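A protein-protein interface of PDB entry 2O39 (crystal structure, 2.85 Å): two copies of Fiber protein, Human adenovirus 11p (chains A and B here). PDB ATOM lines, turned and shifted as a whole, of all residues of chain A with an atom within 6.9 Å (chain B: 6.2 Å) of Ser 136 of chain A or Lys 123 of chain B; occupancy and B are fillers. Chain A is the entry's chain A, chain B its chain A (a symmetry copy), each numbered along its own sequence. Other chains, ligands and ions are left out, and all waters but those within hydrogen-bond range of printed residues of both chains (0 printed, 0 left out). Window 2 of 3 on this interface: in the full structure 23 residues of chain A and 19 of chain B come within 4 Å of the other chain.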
ATOM      1  N   THR A  58      37.199  15.710  -9.277  1.00  0.00           N
ATOM      2  CA  THR A  58      36.832  17.120  -9.169  1.00  0.00           C
ATOM      3  C   THR A  58      38.045  18.038  -9.116  1.00  0.00           C
ATOM      4  O   THR A  58      37.920  19.260  -9.229  1.00  0.00           O
ATOM      5  CB  THR A  58      35.955  17.388  -7.929  1.00  0.00           C
ATOM      6  OG1 THR A  58      36.770  17.387  -6.755  1.00  0.00           O
ATOM      7  CG2 THR A  58      34.897  16.314  -7.793  1.00  0.00           C
ATOM      8  N   TYR A 132      24.678  20.217 -12.594  1.00  0.00           N
ATOM      9  CA  TYR A 132      25.602  21.054 -11.837  1.00  0.00           C
ATOM     10  C   TYR A 132      26.195  20.291 -10.657  1.00  0.00           C
ATOM     11  O   TYR A 132      25.466  19.764  -9.816  1.00  0.00           O
ATOM     12  CB  TYR A 132      24.898  22.320 -11.344  1.00  0.00           C
ATOM     13  CG  TYR A 132      24.325  23.172 -12.454  1.00  0.00           C
ATOM     14  CD1 TYR A 132      23.077  22.892 -12.997  1.00  0.00           C
ATOM     15  CD2 TYR A 132      25.029  24.257 -12.958  1.00  0.00           C
ATOM     16  CE1 TYR A 132      22.549  23.668 -14.012  1.00  0.00           C
ATOM     17  CE2 TYR A 132      24.509  25.039 -13.971  1.00  0.00           C
ATOM     18  CZ  TYR A 132      23.269  24.740 -14.494  1.00  0.00           C
ATOM     19  OH  TYR A 132      22.746  25.516 -15.504  1.00  0.00           O
ATOM     20  N   TYR A 133      27.521  20.236 -10.601  1.00  0.00           N
ATOM     21  CA  TYR A 133      28.224  19.916  -9.364  1.00  0.00           C
ATOM     22  C   TYR A 133      28.325  21.139  -8.457  1.00  0.00           C
ATOM     23  O   TYR A 133      28.865  22.172  -8.850  1.00  0.00           O
ATOM     24  CB  TYR A 133      29.620  19.368  -9.666  1.00  0.00           C
ATOM     25  CG  TYR A 133      30.574  19.447  -8.496  1.00  0.00           C
ATOM     26  CD1 TYR A 133      30.669  18.408  -7.580  1.00  0.00           C
ATOM     27  CD2 TYR A 133      31.383  20.561  -8.309  1.00  0.00           C
ATOM     28  CE1 TYR A 133      31.540  18.475  -6.510  1.00  0.00           C
ATOM     29  CE2 TYR A 133      32.258  20.637  -7.242  1.00  0.00           C
ATOM     30  CZ  TYR A 133      32.332  19.591  -6.345  1.00  0.00           C
ATOM     31  OH  TYR A 133      33.202  19.663  -5.281  1.00  0.00           O
ATOM     32  N   THR A 134      27.802  21.012  -7.241  1.00  0.00           N
ATOM     33  CA  THR A 134      27.822  22.102  -6.287  1.00  0.00           C
ATOM     34  C   THR A 134      29.102  22.006  -5.461  1.00  0.00           C
ATOM     35  O   THR A 134      29.249  21.169  -4.576  1.00  0.00           O
ATOM     36  CB  THR A 134      26.515  22.122  -5.422  1.00  0.00           C
ATOM     37  OG1 THR A 134      26.835  22.270  -4.036  1.00  0.00           O
ATOM     38  CG2 THR A 134      25.696  20.865  -5.658  1.00  0.00           C
ATOM     39  N   ALA A 135      30.039  22.878  -5.811  1.00  0.00           N
ATOM     40  CA  ALA A 135      31.343  22.960  -5.182  1.00  0.00           C
ATOM     41  C   ALA A 135      31.371  23.430  -3.732  1.00  0.00           C
ATOM     42  O   ALA A 135      30.393  23.966  -3.198  1.00  0.00           O
ATOM     43  CB  ALA A 135      32.229  23.861  -6.002  1.00  0.00           C
ATOM     44  N   SER A 136      32.541  23.247  -3.127  1.00  0.00           N
ATOM     45  CA  SER A 136      32.818  23.625  -1.753  1.00  0.00           C
ATOM     46  C   SER A 136      32.411  25.073  -1.437  1.00  0.00           C
ATOM     47  O   SER A 136      31.587  25.314  -0.555  1.00  0.00           O
ATOM     48  CB  SER A 136      34.311  23.425  -1.490  1.00  0.00           C
ATOM     49  OG  SER A 136      34.598  23.426  -0.104  1.00  0.00           O
ATOM     50  N   ASP A 137      32.985  26.036  -2.150  1.00  0.00           N
ATOM     51  CA  ASP A 137      32.656  27.440  -1.922  1.00  0.00           C
ATOM     52  C   ASP A 137      31.228  27.752  -2.336  1.00  0.00           C
ATOM     53  O   ASP A 137      30.874  28.911  -2.544  1.00  0.00           O
ATOM     54  CB  ASP A 137      33.622  28.349  -2.686  1.00  0.00           C
ATOM     55  CG  ASP A 137      33.675  28.024  -4.148  1.00  0.00           C
ATOM     56  OD1 ASP A 137      32.781  27.286  -4.601  1.00  0.00           O
ATOM     57  OD2 ASP A 137      34.596  28.504  -4.844  1.00  0.00           O
ATOM     58  N   ARG A 138      30.420  26.701  -2.469  1.00  0.00           N
ATOM     59  CA  ARG A 138      29.007  26.807  -2.843  1.00  0.00           C
ATOM     60  C   ARG A 138      28.651  27.279  -4.264  1.00  0.00           C
ATOM     61  O   ARG A 138      27.472  27.481  -4.573  1.00  0.00           O
ATOM     62  CB  ARG A 138      28.267  27.672  -1.813  1.00  0.00           C
ATOM     63  CG  ARG A 138      27.944  26.914  -0.537  1.00  0.00           C
ATOM     64  CD  ARG A 138      27.490  27.836   0.594  1.00  0.00           C
ATOM     65  NE  ARG A 138      27.191  27.068   1.799  1.00  0.00           N
ATOM     66  CZ  ARG A 138      26.124  26.284   1.933  1.00  0.00           C
ATOM     67  NH1 ARG A 138      25.249  26.177   0.937  1.00  0.00           N
ATOM     68  NH2 ARG A 138      25.952  25.580   3.049  1.00  0.00           N
ATOM     69  N   THR A 139      29.644  27.450  -5.131  1.00  0.00           N
ATOM     70  CA  THR A 139      29.355  27.872  -6.491  1.00  0.00           C
ATOM     71  C   THR A 139      28.848  26.690  -7.302  1.00  0.00           C
ATOM     72  O   THR A 139      29.157  25.538  -6.990  1.00  0.00           O
ATOM     73  CB  THR A 139      30.594  28.447  -7.188  1.00  0.00           C
ATOM     74  OG1 THR A 139      31.760  28.074  -6.458  1.00  0.00           O
ATOM     75  CG2 THR A 139      30.513  29.966  -7.274  1.00  0.00           C
ATOM     76  N   PRO A 174      36.927  22.115 -10.820  1.00  0.00           N
ATOM     77  CA  PRO A 174      35.889  22.544  -9.885  1.00  0.00           C
ATOM     78  C   PRO A 174      36.277  22.403  -8.423  1.00  0.00           C
ATOM     79  O   PRO A 174      35.477  22.714  -7.550  1.00  0.00           O
ATOM     80  CB  PRO A 174      34.710  21.658 -10.257  1.00  0.00           C
ATOM     81  CG  PRO A 174      35.372  20.407 -10.681  1.00  0.00           C
ATOM     82  CD  PRO A 174      36.500  20.907 -11.544  1.00  0.00           C
ATOM     83  N   GLU A 175      37.497  21.935  -8.161  1.00  0.00           N
ATOM     84  CA  GLU A 175      37.977  21.759  -6.789  1.00  0.00           C
ATOM     85  C   GLU A 175      39.500  21.764  -6.650  1.00  0.00           C
ATOM     86  O   GLU A 175      40.239  21.835  -7.628  1.00  0.00           O
ATOM     87  CB  GLU A 175      37.448  20.444  -6.193  1.00  0.00           C
ATOM     88  CG  GLU A 175      35.978  20.440  -5.777  1.00  0.00           C
ATOM     89  CD  GLU A 175      35.634  21.538  -4.787  1.00  0.00           C
ATOM     90  OE1 GLU A 175      36.561  22.194  -4.271  1.00  0.00           O
ATOM     91  OE2 GLU A 175      34.433  21.743  -4.521  1.00  0.00           O
ATOM     92  N   THR A 178      42.768  20.444  -0.964  1.00  0.00           N
ATOM     93  CA  THR A 178      42.237  20.716   0.368  1.00  0.00           C
ATOM     94  C   THR A 178      40.726  20.833   0.496  1.00  0.00           C
ATOM     95  O   THR A 178      40.189  20.694   1.591  1.00  0.00           O
ATOM     96  CB  THR A 178      42.850  22.010   0.955  1.00  0.00           C
ATOM     97  OG1 THR A 178      42.446  23.133   0.165  1.00  0.00           O
ATOM     98  CG2 THR A 178      44.368  21.933   0.961  1.00  0.00           C
ATOM     99  N   SER A 179      40.036  21.078  -0.611  1.00  0.00           N
ATOM    100  CA  SER A 179      38.588  21.249  -0.560  1.00  0.00           C
ATOM    101  C   SER A 179      37.772  20.082  -1.079  1.00  0.00           C
ATOM    102  O   SER A 179      36.614  19.922  -0.700  1.00  0.00           O
ATOM    103  CB  SER A 179      38.201  22.500  -1.335  1.00  0.00           C
ATOM    104  OG  SER A 179      38.691  22.423  -2.666  1.00  0.00           O
ATOM    105  N   ALA A 180      38.360  19.278  -1.955  1.00  0.00           N
ATOM    106  CA  ALA A 180      37.648  18.135  -2.510  1.00  0.00           C
ATOM    107  C   ALA A 180      36.979  17.270  -1.435  1.00  0.00           C
ATOM    108  O   ALA A 180      37.399  17.262  -0.273  1.00  0.00           O
ATOM    109  CB  ALA A 180      38.593  17.296  -3.330  1.00  0.00           C
ATOM    110  N   THR A 181      35.941  16.543  -1.847  1.00  0.00           N
ATOM    111  CA  THR A 181      35.173  15.657  -0.972  1.00  0.00           C
ATOM    112  C   THR A 181      34.519  14.545  -1.816  1.00  0.00           C
ATOM    113  O   THR A 181      35.153  13.534  -2.141  1.00  0.00           O
ATOM    114  CB  THR A 181      34.081  16.452  -0.229  1.00  0.00           C
ATOM    115  OG1 THR A 181      33.371  17.270  -1.168  1.00  0.00           O
ATOM    116  CG2 THR A 181      34.694  17.347   0.833  1.00  0.00           C
ATOM    117  N   THR A 182      33.254  14.736  -2.176  1.00  0.00           N
ATOM    118  CA  THR A 182      32.540  13.763  -2.998  1.00  0.00           C
ATOM    119  C   THR A 182      32.157  14.375  -4.335  1.00  0.00           C
ATOM    120  O   THR A 182      31.941  15.581  -4.433  1.00  0.00           O
ATOM    121  CB  THR A 182      31.241  13.292  -2.339  1.00  0.00           C
ATOM    122  OG1 THR A 182      31.544  12.570  -1.139  1.00  0.00           O
ATOM    123  CG2 THR A 182      30.477  12.390  -3.283  1.00  0.00           C
ATOM    124  N   LEU A 183      32.081  13.541  -5.366  1.00  0.00           N
ATOM    125  CA  LEU A 183      31.694  13.999  -6.692  1.00  0.00           C
ATOM    126  C   LEU A 183      30.221  13.668  -6.821  1.00  0.00           C
ATOM    127  O   LEU A 183      29.836  12.497  -6.856  1.00  0.00           O
ATOM    128  CB  LEU A 183      32.496  13.280  -7.776  1.00  0.00           C
ATOM    129  CG  LEU A 183      32.057  13.507  -9.226  1.00  0.00           C
ATOM    130  CD1 LEU A 183      32.067  14.980  -9.582  1.00  0.00           C
ATOM    131  CD2 LEU A 183      32.989  12.735 -10.137  1.00  0.00           C
ATOM    132  N   VAL A 184      29.402  14.712  -6.873  1.00  0.00           N
ATOM    133  CA  VAL A 184      27.959  14.561  -6.969  1.00  0.00           C
ATOM    134  C   VAL A 184      27.373  15.440  -8.058  1.00  0.00           C
ATOM    135  O   VAL A 184      27.698  16.619  -8.154  1.00  0.00           O
ATOM    136  CB  VAL A 184      27.284  14.945  -5.631  1.00  0.00           C
ATOM    137  CG1 VAL A 184      25.776  15.044  -5.805  1.00  0.00           C
ATOM    138  CG2 VAL A 184      27.632  13.926  -4.568  1.00  0.00           C
ATOM    139  N   THR A 185      26.511  14.868  -8.882  1.00  0.00           N
ATOM    140  CA  THR A 185      25.867  15.652  -9.924  1.00  0.00           C
ATOM    141  C   THR A 185      24.441  15.931  -9.473  1.00  0.00           C
ATOM    142  O   THR A 185      23.885  15.208  -8.638  1.00  0.00           O
ATOM    143  CB  THR A 185      25.820  14.903 -11.284  1.00  0.00           C
ATOM    144  OG1 THR A 185      25.164  13.636 -11.121  1.00  0.00           O
ATOM    145  CG2 THR A 185      27.233  14.696 -11.825  1.00  0.00           C
ATOM    146  N   SER A 186      23.853  16.997  -9.999  1.00  0.00           N
ATOM    147  CA  SER A 186      22.490  17.316  -9.639  1.00  0.00           C
ATOM    148  C   SER A 186      21.601  16.488 -10.554  1.00  0.00           C
ATOM    149  O   SER A 186      22.012  16.098 -11.661  1.00  0.00           O
ATOM    150  CB  SER A 186      22.222  18.809  -9.813  1.00  0.00           C
ATOM    151  OG  SER A 186      22.626  19.265 -11.083  1.00  0.00           O
ATOM    152  N   ASP B 118      23.233  16.528   7.140  1.00  0.00           N
ATOM    153  CA  ASP B 118      24.203  15.493   6.812  1.00  0.00           C
ATOM    154  C   ASP B 118      25.199  16.172   5.884  1.00  0.00           C
ATOM    155  O   ASP B 118      24.971  16.273   4.675  1.00  0.00           O
ATOM    156  CB  ASP B 118      23.557  14.306   6.100  1.00  0.00           C
ATOM    157  CG  ASP B 118      24.530  13.160   5.894  1.00  0.00           C
ATOM    158  OD1 ASP B 118      25.738  13.461   5.790  1.00  0.00           O
ATOM    159  OD2 ASP B 118      24.103  11.974   5.826  1.00  0.00           O
ATOM    160  N   ASN B 119      26.292  16.656   6.463  1.00  0.00           N
ATOM    161  CA  ASN B 119      27.313  17.345   5.695  1.00  0.00           C
ATOM    162  C   ASN B 119      28.025  16.488   4.678  1.00  0.00           C
ATOM    163  O   ASN B 119      28.631  17.014   3.744  1.00  0.00           O
ATOM    164  CB  ASN B 119      28.319  17.986   6.632  1.00  0.00           C
ATOM    165  CG  ASN B 119      27.762  19.209   7.288  1.00  0.00           C
ATOM    166  OD1 ASN B 119      26.552  19.297   7.512  1.00  0.00           O
ATOM    167  ND2 ASN B 119      28.627  20.166   7.602  1.00  0.00           N
ATOM    168  N   SER B 120      27.950  15.173   4.842  1.00  0.00           N
ATOM    169  CA  SER B 120      28.602  14.281   3.890  1.00  0.00           C
ATOM    170  C   SER B 120      27.746  14.112   2.624  1.00  0.00           C
ATOM    171  O   SER B 120      28.231  13.652   1.584  1.00  0.00           O
ATOM    172  CB  SER B 120      28.873  12.913   4.534  1.00  0.00           C
ATOM    173  OG  SER B 120      27.669  12.228   4.842  1.00  0.00           O
ATOM    174  N   ARG B 121      26.473  14.495   2.716  1.00  0.00           N
ATOM    175  CA  ARG B 121      25.554  14.380   1.586  1.00  0.00           C
ATOM    176  C   ARG B 121      24.957  15.722   1.182  1.00  0.00           C
ATOM    177  O   ARG B 121      24.073  15.792   0.346  1.00  0.00           O
ATOM    178  CB  ARG B 121      24.445  13.398   1.935  1.00  0.00           C
ATOM    179  CG  ARG B 121      24.973  12.020   2.265  1.00  0.00           C
ATOM    180  CD  ARG B 121      23.837  11.106   2.593  1.00  0.00           C
ATOM    181  NE  ARG B 121      22.809  11.182   1.568  1.00  0.00           N
ATOM    182  CZ  ARG B 121      21.580  10.707   1.718  1.00  0.00           C
ATOM    183  NH1 ARG B 121      21.234  10.120   2.856  1.00  0.00           N
ATOM    184  NH2 ARG B 121      20.697  10.836   0.732  1.00  0.00           N
ATOM    185  N   GLU B 122      25.458  16.785   1.796  1.00  0.00           N
ATOM    186  CA  GLU B 122      25.004  18.128   1.513  1.00  0.00           C
ATOM    187  C   GLU B 122      24.839  18.399   0.030  1.00  0.00           C
ATOM    188  O   GLU B 122      23.768  18.825  -0.415  1.00  0.00           O
ATOM    189  CB  GLU B 122      25.988  19.138   2.096  1.00  0.00           C
ATOM    190  CG  GLU B 122      25.978  20.478   1.379  1.00  0.00           C
ATOM    191  CD  GLU B 122      26.857  21.509   2.056  1.00  0.00           C
ATOM    192  OE1 GLU B 122      28.061  21.224   2.259  1.00  0.00           O
ATOM    193  OE2 GLU B 122      26.337  22.603   2.385  1.00  0.00           O
ATOM    194  N   LYS B 123      25.890  18.160  -0.745  1.00  0.00           N
ATOM    195  CA  LYS B 123      25.813  18.435  -2.176  1.00  0.00           C
ATOM    196  C   LYS B 123      24.535  17.909  -2.821  1.00  0.00           C
ATOM    197  O   LYS B 123      24.037  18.494  -3.771  1.00  0.00           O
ATOM    198  CB  LYS B 123      27.028  17.853  -2.895  1.00  0.00           C
ATOM    199  CG  LYS B 123      28.346  18.466  -2.467  1.00  0.00           C
ATOM    200  CD  LYS B 123      29.505  17.829  -3.212  1.00  0.00           C
ATOM    201  CE  LYS B 123      30.855  18.296  -2.682  1.00  0.00           C
ATOM    202  NZ  LYS B 123      31.076  19.764  -2.851  1.00  0.00           N
ATOM    203  N   GLU B 124      24.003  16.814  -2.287  1.00  0.00           N
ATOM    204  CA  GLU B 124      22.799  16.184  -2.809  1.00  0.00           C
ATOM    205  C   GLU B 124      21.495  16.932  -2.552  1.00  0.00           C
ATOM    206  O   GLU B 124      20.441  16.505  -3.028  1.00  0.00           O
ATOM    207  CB  GLU B 124      22.676  14.783  -2.231  1.00  0.00           C
ATOM    208  CG  GLU B 124      23.911  13.942  -2.419  1.00  0.00           C
ATOM    209  CD  GLU B 124      23.855  12.653  -1.616  1.00  0.00           C
ATOM    210  OE1 GLU B 124      22.771  12.020  -1.602  1.00  0.00           O
ATOM    211  OE2 GLU B 124      24.886  12.271  -1.012  1.00  0.00           O
ATOM    212  N   ASN B 125      21.563  18.034  -1.803  1.00  0.00           N
ATOM    213  CA  ASN B 125      20.377  18.836  -1.468  1.00  0.00           C
ATOM    214  C   ASN B 125      20.113  19.990  -2.438  1.00  0.00           C
ATOM    215  O   ASN B 125      19.247  20.824  -2.188  1.00  0.00           O
ATOM    216  CB  ASN B 125      20.520  19.437  -0.066  1.00  0.00           C
ATOM    217  CG  ASN B 125      20.454  18.399   1.041  1.00  0.00           C
ATOM    218  OD1 ASN B 125      21.484  17.883   1.508  1.00  0.00           O
ATOM    219  ND2 ASN B 125      19.232  18.084   1.472  1.00  0.00           N
ATOM    220  N   TYR B 126      20.841  20.045  -3.547  1.00  0.00           N
ATOM    221  CA  TYR B 126      20.671  21.145  -4.484  1.00  0.00           C
ATOM    222  C   TYR B 126      20.169  20.826  -5.903  1.00  0.00           C
ATOM    223  O   TYR B 126      20.471  19.777  -6.496  1.00  0.00           O
ATOM    224  CB  TYR B 126      21.981  21.920  -4.577  1.00  0.00           C
ATOM    225  CG  TYR B 126      22.463  22.431  -3.244  1.00  0.00           C
ATOM    226  CD1 TYR B 126      23.460  21.765  -2.523  1.00  0.00           C
ATOM    227  CD2 TYR B 126      21.919  23.589  -2.692  1.00  0.00           C
ATOM    228  CE1 TYR B 126      23.900  22.254  -1.287  1.00  0.00           C
ATOM    229  CE2 TYR B 126      22.348  24.081  -1.463  1.00  0.00           C
ATOM    230  CZ  TYR B 126      23.333  23.421  -0.766  1.00  0.00           C
ATOM    231  OH  TYR B 126      23.751  23.956   0.437  1.00  0.00           O
ATOM    232  N   TYR B 128      19.533  23.126  -9.612  1.00  0.00           N
ATOM    233  CA  TYR B 128      19.771  24.392 -10.297  1.00  0.00           C
ATOM    234  C   TYR B 128      19.075  24.426 -11.652  1.00  0.00           C
ATOM    235  O   TYR B 128      18.700  23.386 -12.194  1.00  0.00           O
ATOM    236  CB  TYR B 128      21.273  24.632 -10.470  1.00  0.00           C
ATOM    237  CG  TYR B 128      22.055  24.573  -9.178  1.00  0.00           C
ATOM    238  CD1 TYR B 128      22.359  23.356  -8.582  1.00  0.00           C
ATOM    239  CD2 TYR B 128      22.491  25.735  -8.552  1.00  0.00           C
ATOM    240  CE1 TYR B 128      23.074  23.297  -7.401  1.00  0.00           C
ATOM    241  CE2 TYR B 128      23.207  25.685  -7.372  1.00  0.00           C
ATOM    242  CZ  TYR B 128      23.495  24.465  -6.801  1.00  0.00           C
ATOM    243  OH  TYR B 128      24.208  24.410  -5.625  1.00  0.00           O
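OH of Tyr 133 of chain A sits at hydrogen-bond distance from NZ of Lys 123 of chain B (3.2 Å). The side-chain amino group of Lys 123 of chain B lies within hydrogen-bond range of the backbone carbonyl oxygen of Thr 134 of chain A, at 2.9 Å. NH2 of Arg 138 of chain A lies within salt-bridge range of OE2 of Glu 122 of chain B. NH1 of Arg 138 of chain A lies within hydrogen-bond range of OH of Tyr 126 of chain B (2.7 Å).
The side-chain hydroxyl (OG) of Ser 186 of chain A is in hydrogen-bond range of the backbone NH (N) of Tyr 132 of chain A. OH of Tyr 133 of chain A lies within hydrogen-bond range of OE2 of Glu 175 of chain A (2.5 Å). N of Ser 136 of chain A lies within hydrogen-bond range of OE2 of Glu 175 of chain A (2.8 Å). O of Glu 122 of chain B lies close to OD1 of Asn 125 of chain B (3.1 Å).
Tyr 132 of chain A touches Tyr 128 of chain B (CD1 to CB, 3.6 Å). CD1 of Tyr 126 of chain B touches OG1 of Thr 134 of chain A (3.7 Å). OH of Tyr 128 of chain B touches CB of Thr 134 of chain A (3.3 Å). Lys 123 of chain B touches Ala 135 of chain A. N of Ser 136 of chain A touches NZ of Lys 123 of chain B, at 3.8 Å. Lys 123 of chain B touches Thr 181 of chain A (CE to OG1, 3.1 Å). O of Thr 182 of chain A touches CE of Lys 123 of chain B, at 3.4 Å. Ser 186 of chain A touches Tyr 126 of chain B.
Of the printed residues of chain B, Tyr 133 of chain A touches Lys 123. Printed residues of chain B within 4 Å of Thr 134 of chain A: Lys 123, Tyr 126 and Tyr 128. Ser 136 of chain A touches one residue of chain B. Ser 179 of chain A touches none of the printed residues of chain B. Asn 125 of chain B touches none of the printed residues of chain A. The nearest printed residue of chain B that does not touch Arg 138 of chain A is Tyr 128 of chain B (4.6 Å).
Of the 20 printed residues of chain A, 9 touch a printed residue of chain B. Printed residues of chain A that touch a printed residue of chain B: Tyr 132, Tyr 133, Thr 134, Ala 135, Ser 136, Arg 138, Thr 181, Thr 182 and Ser 186. Of the 10 printed residues of chain B, 4 touch a printed residue of chain A. Printed residues of chain B that touch a printed residue of chain A: Glu 122, Lys 123, Tyr 126 and Tyr 128. Hydrophobic or aromatic side chains of chain B within 4 Å of the printed part of chain A: Tyr 126 and Tyr 128. Among the printed residues, Asp or Glu carboxylates within 4 Å of a Lys or Arg side-chain nitrogen of the other chain: Arg 138 of chain A with Glu 122 of chain B (3.1 Å).
No position is printed for both chains. Of the 12 pairs that touch across the chains among the printed residues, none has its exchanged pair printed and touching as well.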
